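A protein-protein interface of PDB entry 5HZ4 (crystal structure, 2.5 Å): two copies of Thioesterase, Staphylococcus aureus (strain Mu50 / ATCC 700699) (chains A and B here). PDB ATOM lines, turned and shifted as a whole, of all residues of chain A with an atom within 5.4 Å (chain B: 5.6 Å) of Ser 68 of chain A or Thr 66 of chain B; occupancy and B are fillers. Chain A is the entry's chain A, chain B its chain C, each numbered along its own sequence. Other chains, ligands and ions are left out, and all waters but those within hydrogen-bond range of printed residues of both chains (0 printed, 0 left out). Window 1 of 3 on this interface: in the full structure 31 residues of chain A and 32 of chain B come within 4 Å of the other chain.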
ATOM      1  N   MET A  42      -4.144 -12.317  -9.684  1.00  0.00           N
ATOM      2  CA  MET A  42      -4.386 -12.259 -11.117  1.00  0.00           C
ATOM      3  C   MET A  42      -5.318 -11.108 -11.510  1.00  0.00           C
ATOM      4  O   MET A  42      -5.133 -10.503 -12.545  1.00  0.00           O
ATOM      5  CB  MET A  42      -4.940 -13.595 -11.614  1.00  0.00           C
ATOM      6  CG  MET A  42      -3.867 -14.653 -11.837  1.00  0.00           C
ATOM      7  SD  MET A  42      -4.462 -16.176 -12.620  1.00  0.00           S
ATOM      8  CE  MET A  42      -5.231 -16.999 -11.216  1.00  0.00           C
ATOM      9  N   THR A  66      -4.013 -14.289 -21.268  1.00  0.00           N
ATOM     10  CA  THR A  66      -3.026 -14.282 -20.202  1.00  0.00           C
ATOM     11  C   THR A  66      -2.090 -15.399 -20.532  1.00  0.00           C
ATOM     12  O   THR A  66      -2.484 -16.569 -20.513  1.00  0.00           O
ATOM     13  CB  THR A  66      -3.665 -14.492 -18.829  1.00  0.00           C
ATOM     14  OG1 THR A  66      -4.481 -13.362 -18.516  1.00  0.00           O
ATOM     15  CG2 THR A  66      -2.606 -14.692 -17.742  1.00  0.00           C
ATOM     16  N   ASP A  67      -0.866 -15.042 -20.888  1.00  0.00           N
ATOM     17  CA  ASP A  67       0.056 -16.014 -21.465  1.00  0.00           C
ATOM     18  C   ASP A  67       0.754 -16.862 -20.393  1.00  0.00           C
ATOM     19  O   ASP A  67       1.112 -18.014 -20.649  1.00  0.00           O
ATOM     20  CB  ASP A  67       1.057 -15.302 -22.370  1.00  0.00           C
ATOM     21  CG  ASP A  67       0.360 -14.405 -23.403  1.00  0.00           C
ATOM     22  OD1 ASP A  67      -0.696 -14.805 -23.936  1.00  0.00           O
ATOM     23  OD2 ASP A  67       0.853 -13.292 -23.677  1.00  0.00           O
ATOM     24  N   SER A  68       0.968 -16.284 -19.218  1.00  0.00           N
ATOM     25  CA  SER A  68       1.359 -17.053 -18.041  1.00  0.00           C
ATOM     26  C   SER A  68       1.372 -16.200 -16.789  1.00  0.00           C
ATOM     27  O   SER A  68       1.499 -14.984 -16.830  1.00  0.00           O
ATOM     28  CB  SER A  68       2.726 -17.710 -18.191  1.00  0.00           C
ATOM     29  OG  SER A  68       3.731 -16.736 -18.272  1.00  0.00           O
ATOM     30  N   VAL A  69       1.178 -16.862 -15.667  1.00  0.00           N
ATOM     31  CA  VAL A  69       1.490 -16.281 -14.385  1.00  0.00           C
ATOM     32  C   VAL A  69       2.323 -17.310 -13.618  1.00  0.00           C
ATOM     33  O   VAL A  69       1.845 -18.397 -13.333  1.00  0.00           O
ATOM     34  CB  VAL A  69       0.226 -15.920 -13.582  1.00  0.00           C
ATOM     35  CG1 VAL A  69       0.612 -15.337 -12.214  1.00  0.00           C
ATOM     36  CG2 VAL A  69      -0.690 -14.981 -14.374  1.00  0.00           C
ATOM     37  N   ASP A  70       3.564 -16.966 -13.298  1.00  0.00           N
ATOM     38  CA  ASP A  70       4.396 -17.826 -12.478  1.00  0.00           C
ATOM     39  C   ASP A  70       4.396 -17.371 -11.021  1.00  0.00           C
ATOM     40  O   ASP A  70       4.738 -16.230 -10.730  1.00  0.00           O
ATOM     41  CB  ASP A  70       5.819 -17.848 -13.010  1.00  0.00           C
ATOM     42  CG  ASP A  70       6.010 -18.872 -14.094  1.00  0.00           C
ATOM     43  OD1 ASP A  70       6.249 -18.474 -15.246  1.00  0.00           O
ATOM     44  OD2 ASP A  70       5.852 -20.076 -13.812  1.00  0.00           O
ATOM     45  N   PHE A  71       3.973 -18.251 -10.120  1.00  0.00           N
ATOM     46  CA  PHE A  71       4.035 -17.976  -8.676  1.00  0.00           C
ATOM     47  C   PHE A  71       5.356 -18.494  -8.124  1.00  0.00           C
ATOM     48  O   PHE A  71       5.609 -19.704  -8.120  1.00  0.00           O
ATOM     49  CB  PHE A  71       2.841 -18.597  -7.945  1.00  0.00           C
ATOM     50  CG  PHE A  71       1.507 -18.081  -8.437  1.00  0.00           C
ATOM     51  CD1 PHE A  71       0.706 -18.840  -9.276  1.00  0.00           C
ATOM     52  CD2 PHE A  71       1.067 -16.824  -8.090  1.00  0.00           C
ATOM     53  CE1 PHE A  71      -0.518 -18.360  -9.724  1.00  0.00           C
ATOM     54  CE2 PHE A  71      -0.165 -16.354  -8.551  1.00  0.00           C
ATOM     55  CZ  PHE A  71      -0.947 -17.123  -9.353  1.00  0.00           C
ATOM     56  N   LEU A 116       5.556 -13.394 -11.540  1.00  0.00           N
ATOM     57  CA  LEU A 116       5.877 -12.828 -12.847  1.00  0.00           C
ATOM     58  C   LEU A 116       4.798 -13.218 -13.836  1.00  0.00           C
ATOM     59  O   LEU A 116       4.421 -14.389 -13.903  1.00  0.00           O
ATOM     60  CB  LEU A 116       7.216 -13.352 -13.356  1.00  0.00           C
ATOM     61  CG  LEU A 116       7.772 -12.606 -14.561  1.00  0.00           C
ATOM     62  CD1 LEU A 116       8.067 -11.145 -14.174  1.00  0.00           C
ATOM     63  CD2 LEU A 116       8.981 -13.306 -15.181  1.00  0.00           C
ATOM     64  N   SER A 117       4.300 -12.260 -14.614  1.00  0.00           N
ATOM     65  CA  SER A 117       3.208 -12.556 -15.526  1.00  0.00           C
ATOM     66  C   SER A 117       3.360 -11.878 -16.889  1.00  0.00           C
ATOM     67  O   SER A 117       3.859 -10.739 -16.999  1.00  0.00           O
ATOM     68  CB  SER A 117       1.876 -12.143 -14.886  1.00  0.00           C
ATOM     69  OG  SER A 117       0.781 -12.612 -15.679  1.00  0.00           O
ATOM     70  N   TYR A 118       2.883 -12.555 -17.932  1.00  0.00           N
ATOM     71  CA  TYR A 118       2.888 -11.962 -19.268  1.00  0.00           C
ATOM     72  C   TYR A 118       1.496 -11.980 -19.895  1.00  0.00           C
ATOM     73  O   TYR A 118       0.838 -13.029 -19.920  1.00  0.00           O
ATOM     74  CB  TYR A 118       3.866 -12.709 -20.190  1.00  0.00           C
ATOM     75  CG  TYR A 118       5.319 -12.675 -19.755  1.00  0.00           C
ATOM     76  CD1 TYR A 118       5.885 -13.740 -19.049  1.00  0.00           C
ATOM     77  CD2 TYR A 118       6.133 -11.585 -20.054  1.00  0.00           C
ATOM     78  CE1 TYR A 118       7.218 -13.711 -18.663  1.00  0.00           C
ATOM     79  CE2 TYR A 118       7.456 -11.551 -19.665  1.00  0.00           C
ATOM     80  CZ  TYR A 118       7.997 -12.614 -18.992  1.00  0.00           C
ATOM     81  OH  TYR A 118       9.320 -12.561 -18.605  1.00  0.00           O
ATOM     82  N   ASP B  46      -9.415 -19.486 -11.023  1.00  0.00           N
ATOM     83  CA  ASP B  46      -8.516 -19.912  -9.967  1.00  0.00           C
ATOM     84  C   ASP B  46      -9.212 -20.638  -8.832  1.00  0.00           C
ATOM     85  O   ASP B  46      -8.689 -21.606  -8.290  1.00  0.00           O
ATOM     86  CB  ASP B  46      -7.779 -18.719  -9.388  1.00  0.00           C
ATOM     87  CG  ASP B  46      -6.876 -19.114  -8.256  1.00  0.00           C
ATOM     88  OD1 ASP B  46      -5.880 -19.834  -8.523  1.00  0.00           O
ATOM     89  OD2 ASP B  46      -7.188 -18.729  -7.101  1.00  0.00           O
ATOM     90  N   ALA B  64       1.136 -23.564  -8.591  1.00  0.00           N
ATOM     91  CA  ALA B  64       2.486 -23.273  -9.027  1.00  0.00           C
ATOM     92  C   ALA B  64       2.413 -22.168 -10.085  1.00  0.00           C
ATOM     93  O   ALA B  64       3.153 -21.185 -10.042  1.00  0.00           O
ATOM     94  CB  ALA B  64       3.146 -24.484  -9.585  1.00  0.00           C
ATOM     95  N   SER B  65       1.446 -22.304 -10.982  1.00  0.00           N
ATOM     96  CA  SER B  65       1.345 -21.418 -12.123  1.00  0.00           C
ATOM     97  C   SER B  65       0.005 -21.449 -12.846  1.00  0.00           C
ATOM     98  O   SER B  65      -0.705 -22.475 -12.881  1.00  0.00           O
ATOM     99  CB  SER B  65       2.453 -21.784 -13.109  1.00  0.00           C
ATOM    100  OG  SER B  65       2.289 -23.132 -13.545  1.00  0.00           O
ATOM    101  N   THR B  66      -0.327 -20.307 -13.433  1.00  0.00           N
ATOM    102  CA  THR B  66      -1.371 -20.219 -14.442  1.00  0.00           C
ATOM    103  C   THR B  66      -0.666 -20.249 -15.781  1.00  0.00           C
ATOM    104  O   THR B  66       0.065 -19.307 -16.136  1.00  0.00           O
ATOM    105  CB  THR B  66      -2.198 -18.961 -14.325  1.00  0.00           C
ATOM    106  OG1 THR B  66      -2.982 -19.016 -13.139  1.00  0.00           O
ATOM    107  CG2 THR B  66      -3.130 -18.814 -15.546  1.00  0.00           C
ATOM    108  N   ASP B  67      -0.860 -21.343 -16.505  1.00  0.00           N
ATOM    109  CA  ASP B  67      -0.068 -21.608 -17.703  1.00  0.00           C
ATOM    110  C   ASP B  67      -0.586 -20.889 -18.937  1.00  0.00           C
ATOM    111  O   ASP B  67       0.189 -20.593 -19.837  1.00  0.00           O
ATOM    112  CB  ASP B  67      -0.009 -23.105 -17.953  1.00  0.00           C
ATOM    113  CG  ASP B  67       0.423 -23.851 -16.723  1.00  0.00           C
ATOM    114  OD1 ASP B  67       1.315 -23.341 -16.023  1.00  0.00           O
ATOM    115  OD2 ASP B  67      -0.131 -24.931 -16.428  1.00  0.00           O
ATOM    116  N   SER B  68      -1.900 -20.669 -18.982  1.00  0.00           N
ATOM    117  CA  SER B  68      -2.534 -19.799 -19.970  1.00  0.00           C
ATOM    118  C   SER B  68      -4.006 -19.552 -19.675  1.00  0.00           C
ATOM    119  O   SER B  68      -4.686 -20.371 -19.061  1.00  0.00           O
ATOM    120  CB  SER B  68      -2.432 -20.386 -21.371  1.00  0.00           C
ATOM    121  OG  SER B  68      -3.169 -21.596 -21.437  1.00  0.00           O
ATOM    122  N   VAL B  69      -4.484 -18.401 -20.106  1.00  0.00           N
ATOM    123  CA  VAL B  69      -5.913 -18.158 -20.255  1.00  0.00           C
ATOM    124  C   VAL B  69      -6.106 -17.582 -21.638  1.00  0.00           C
ATOM    125  O   VAL B  69      -5.554 -16.539 -21.949  1.00  0.00           O
ATOM    126  CB  VAL B  69      -6.501 -17.166 -19.208  1.00  0.00           C
ATOM    127  CG1 VAL B  69      -7.986 -16.943 -19.485  1.00  0.00           C
ATOM    128  CG2 VAL B  69      -6.253 -17.652 -17.762  1.00  0.00           C
ATOM    129  N   SER B 117      -8.525 -22.309 -20.125  1.00  0.00           N
ATOM    130  CA  SER B 117      -7.411 -22.042 -19.260  1.00  0.00           C
ATOM    131  C   SER B 117      -6.757 -23.322 -18.747  1.00  0.00           C
ATOM    132  O   SER B 117      -7.436 -24.328 -18.488  1.00  0.00           O
ATOM    133  CB  SER B 117      -7.893 -21.167 -18.099  1.00  0.00           C
ATOM    134  OG  SER B 117      -6.794 -20.719 -17.340  1.00  0.00           O
ATOM    135  N   TYR B 118      -5.440 -23.271 -18.556  1.00  0.00           N
ATOM    136  CA  TYR B 118      -4.729 -24.408 -17.971  1.00  0.00           C
ATOM    137  C   TYR B 118      -3.925 -23.964 -16.753  1.00  0.00           C
ATOM    138  O   TYR B 118      -3.180 -22.981 -16.820  1.00  0.00           O
ATOM    139  CB  TYR B 118      -3.801 -25.059 -19.009  1.00  0.00           C
ATOM    140  CG  TYR B 118      -4.518 -25.682 -20.208  1.00  0.00           C
ATOM    141  CD1 TYR B 118      -4.669 -24.974 -21.408  1.00  0.00           C
ATOM    142  CD2 TYR B 118      -5.065 -26.978 -20.132  1.00  0.00           C
ATOM    143  CE1 TYR B 118      -5.332 -25.543 -22.507  1.00  0.00           C
ATOM    144  CE2 TYR B 118      -5.721 -27.550 -21.211  1.00  0.00           C
ATOM    145  CZ  TYR B 118      -5.845 -26.842 -22.405  1.00  0.00           C
ATOM    146  OH  TYR B 118      -6.518 -27.413 -23.486  1.00  0.00           O
ATOM    147  N   LEU B 119      -4.051 -24.689 -15.644  1.00  0.00           N
ATOM    148  CA  LEU B 119      -3.321 -24.305 -14.440  1.00  0.00           C
ATOM    149  C   LEU B 119      -2.517 -25.447 -13.859  1.00  0.00           C
ATOM    150  O   LEU B 119      -2.769 -26.586 -14.170  1.00  0.00           O
ATOM    151  CB  LEU B 119      -4.263 -23.782 -13.377  1.00  0.00           C
ATOM    152  CG  LEU B 119      -5.092 -22.575 -13.739  1.00  0.00           C
ATOM    153  CD1 LEU B 119      -6.419 -23.001 -14.442  1.00  0.00           C
ATOM    154  CD2 LEU B 119      -5.371 -21.789 -12.471  1.00  0.00           C
ATOM    155  N   THR B 120      -1.538 -25.129 -13.022  1.00  0.00           N
ATOM    156  CA  THR B 120      -0.712 -26.153 -12.411  1.00  0.00           C
ATOM    157  C   THR B 120      -0.718 -26.087 -10.910  1.00  0.00           C
ATOM    158  O   THR B 120      -0.481 -25.031 -10.366  1.00  0.00           O
ATOM    159  CB  THR B 120       0.715 -26.049 -12.877  1.00  0.00           C
ATOM    160  OG1 THR B 120       0.757 -26.289 -14.284  1.00  0.00           O
ATOM    161  CG2 THR B 120       1.584 -27.059 -12.135  1.00  0.00           C
ATOM    162  N   ARG B 160       9.566 -23.338 -19.635  1.00  0.00           N
ATOM    163  CA  ARG B 160       9.331 -21.924 -19.434  1.00  0.00           C
ATOM    164  C   ARG B 160       9.561 -21.416 -17.993  1.00  0.00           C
ATOM    165  O   ARG B 160       9.804 -20.210 -17.803  1.00  0.00           O
ATOM    166  CB  ARG B 160       7.911 -21.577 -19.906  1.00  0.00           C
ATOM    167  CG  ARG B 160       7.207 -20.607 -19.000  1.00  0.00           C
ATOM    168  CD  ARG B 160       5.775 -20.402 -19.325  1.00  0.00           C
ATOM    169  NE  ARG B 160       5.137 -19.849 -18.147  1.00  0.00           N
ATOM    170  CZ  ARG B 160       4.540 -20.594 -17.224  1.00  0.00           C
ATOM    171  NH1 ARG B 160       4.456 -21.910 -17.379  1.00  0.00           N
ATOM    172  NH2 ARG B 160       3.993 -20.021 -16.161  1.00  0.00           N
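The side-chain sulfur (SD) of Met 42 of chain A is in hydrogen-bond range of the side-chain hydroxyl (OG1) of Thr 66 of chain B, 3.2 Å away.
The backbone NH (N) of Val 69 of chain B lies within hydrogen-bond range of the backbone carbonyl oxygen (O) of Thr 66 of chain A (2.7 Å).
OG of Ser 68 of chain A sits close to NE of Arg 160 of chain B.
N of Val 69 of chain A sits at hydrogen-bond distance from O of Thr 66 of chain B (2.7 Å).
OD1 of Asp 70 of chain A lies within salt-bridge range of NH2 of Arg 160 of chain B (2.9 Å).
The backbone NH (N) of Phe 71 of chain A lies within hydrogen-bond range of the backbone carbonyl oxygen (O) of Ala 64 of chain B, at 3.0 Å.
O of Asp 67 of chain A sits close to O of Asp 67 of chain B (2.9 Å).
N of Asp 67 of chain A sits at hydrogen-bond distance from O of Tyr 118 of chain A.
The side-chain hydroxyl (OG) of Ser 117 of chain A sits at hydrogen-bond distance from the backbone carbonyl oxygen (O) of Ser 68 of chain A, at 2.7 Å.
N of Asp 70 of chain A sits at hydrogen-bond distance from O of Leu 116 of chain A, 2.8 Å away.
The side-chain hydroxyl of Ser 65 of chain B lies within hydrogen-bond range of the side-chain carboxylate of Asp 67 of chain B (2.7 Å).
The backbone carbonyl oxygen (O) of Ser 65 of chain B lies within hydrogen-bond range of the backbone NH (N) of Thr 120 of chain B (2.8 Å).
The side-chain carboxylate of Asp 67 of chain B lies within salt-bridge range of the guanidinium group of Arg 160 of chain B (3.7 Å).
Hydrophobic or aromatic side chains of chain B that line the printed part of chain A: Val 69.
Of the 10 printed residues of chain A, 7 touch a printed residue of chain B.
Along chain A the printed residues that touch a printed residue of chain B span positions 42 to 71.
Among the printed residues, Asp or Glu carboxylates within 4 Å of a Lys or Arg side-chain nitrogen of the other chain: Asp 70 of chain A with Arg 160 of chain B.
Thr 66 of chain A touches Ser 68 of chain B, and with the chains exchanged Ser 68 of chain A touches Thr 66 of chain B.
Thr 66 of chain A touches Val 69 of chain B, and with the chains exchanged Val 69 of chain A touches Thr 66 of chain B.
Asp 67 of chain B touches its own counterpart, Asp 67 of chain A.
Positions printed for both chains: 66, 67, 68, 69, 117 and 118.
Of the 14 pairs that touch across the chains among the printed residues, 5 have their exchanged pair printed and touching as well.
Ser 68 of chain A touches just these residues of chain B: Thr 66 (3.2 Å) and Arg 160 (3.2 Å).
Printed residues of chain B within 4 Å of Asp 67 of chain A: Asp 67 (2.9 Å).
Of the printed residues of chain A, Asp 46 of chain B touches Met 42.
Printed residues of chain B within 4 Å of Thr 66 of chain A: Ser 68 (3.3 Å) and Val 69 (2.7 Å).
Printed residues of chain A within 4 Å of Arg 160 of chain B: Ser 68, Val 69 and Asp 70.
Of the printed residues of chain A, Ser 65 of chain B touches Val 69, Asp 70 and Phe 71.
Tyr 118 of chain A touches none of the printed residues of chain B.
Ser 117 of chain B touches none of the printed residues of chain A.
The nearest residue of chain B that does not touch Ser 68 of chain A is Asp 67 of chain B (4.1 Å).
Met 42 of chain A touches Asp 46 of chain B.
Thr 66 of chain A touches Ser 68 of chain B.
Thr 66 of chain B touches Ser 68 of chain A.
Val 69 of chain A touches Ser 65 of chain B (O to CA, 3.3 Å).
Arg 160 of chain B touches Val 69 of chain A (NH2 to O, 3.9 Å).
Ser 65 of chain B touches Asp 70 of chain A.
CA of Ser 65 of chain B touches CD1 of Phe 71 of chain A, 3.9 Å away.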
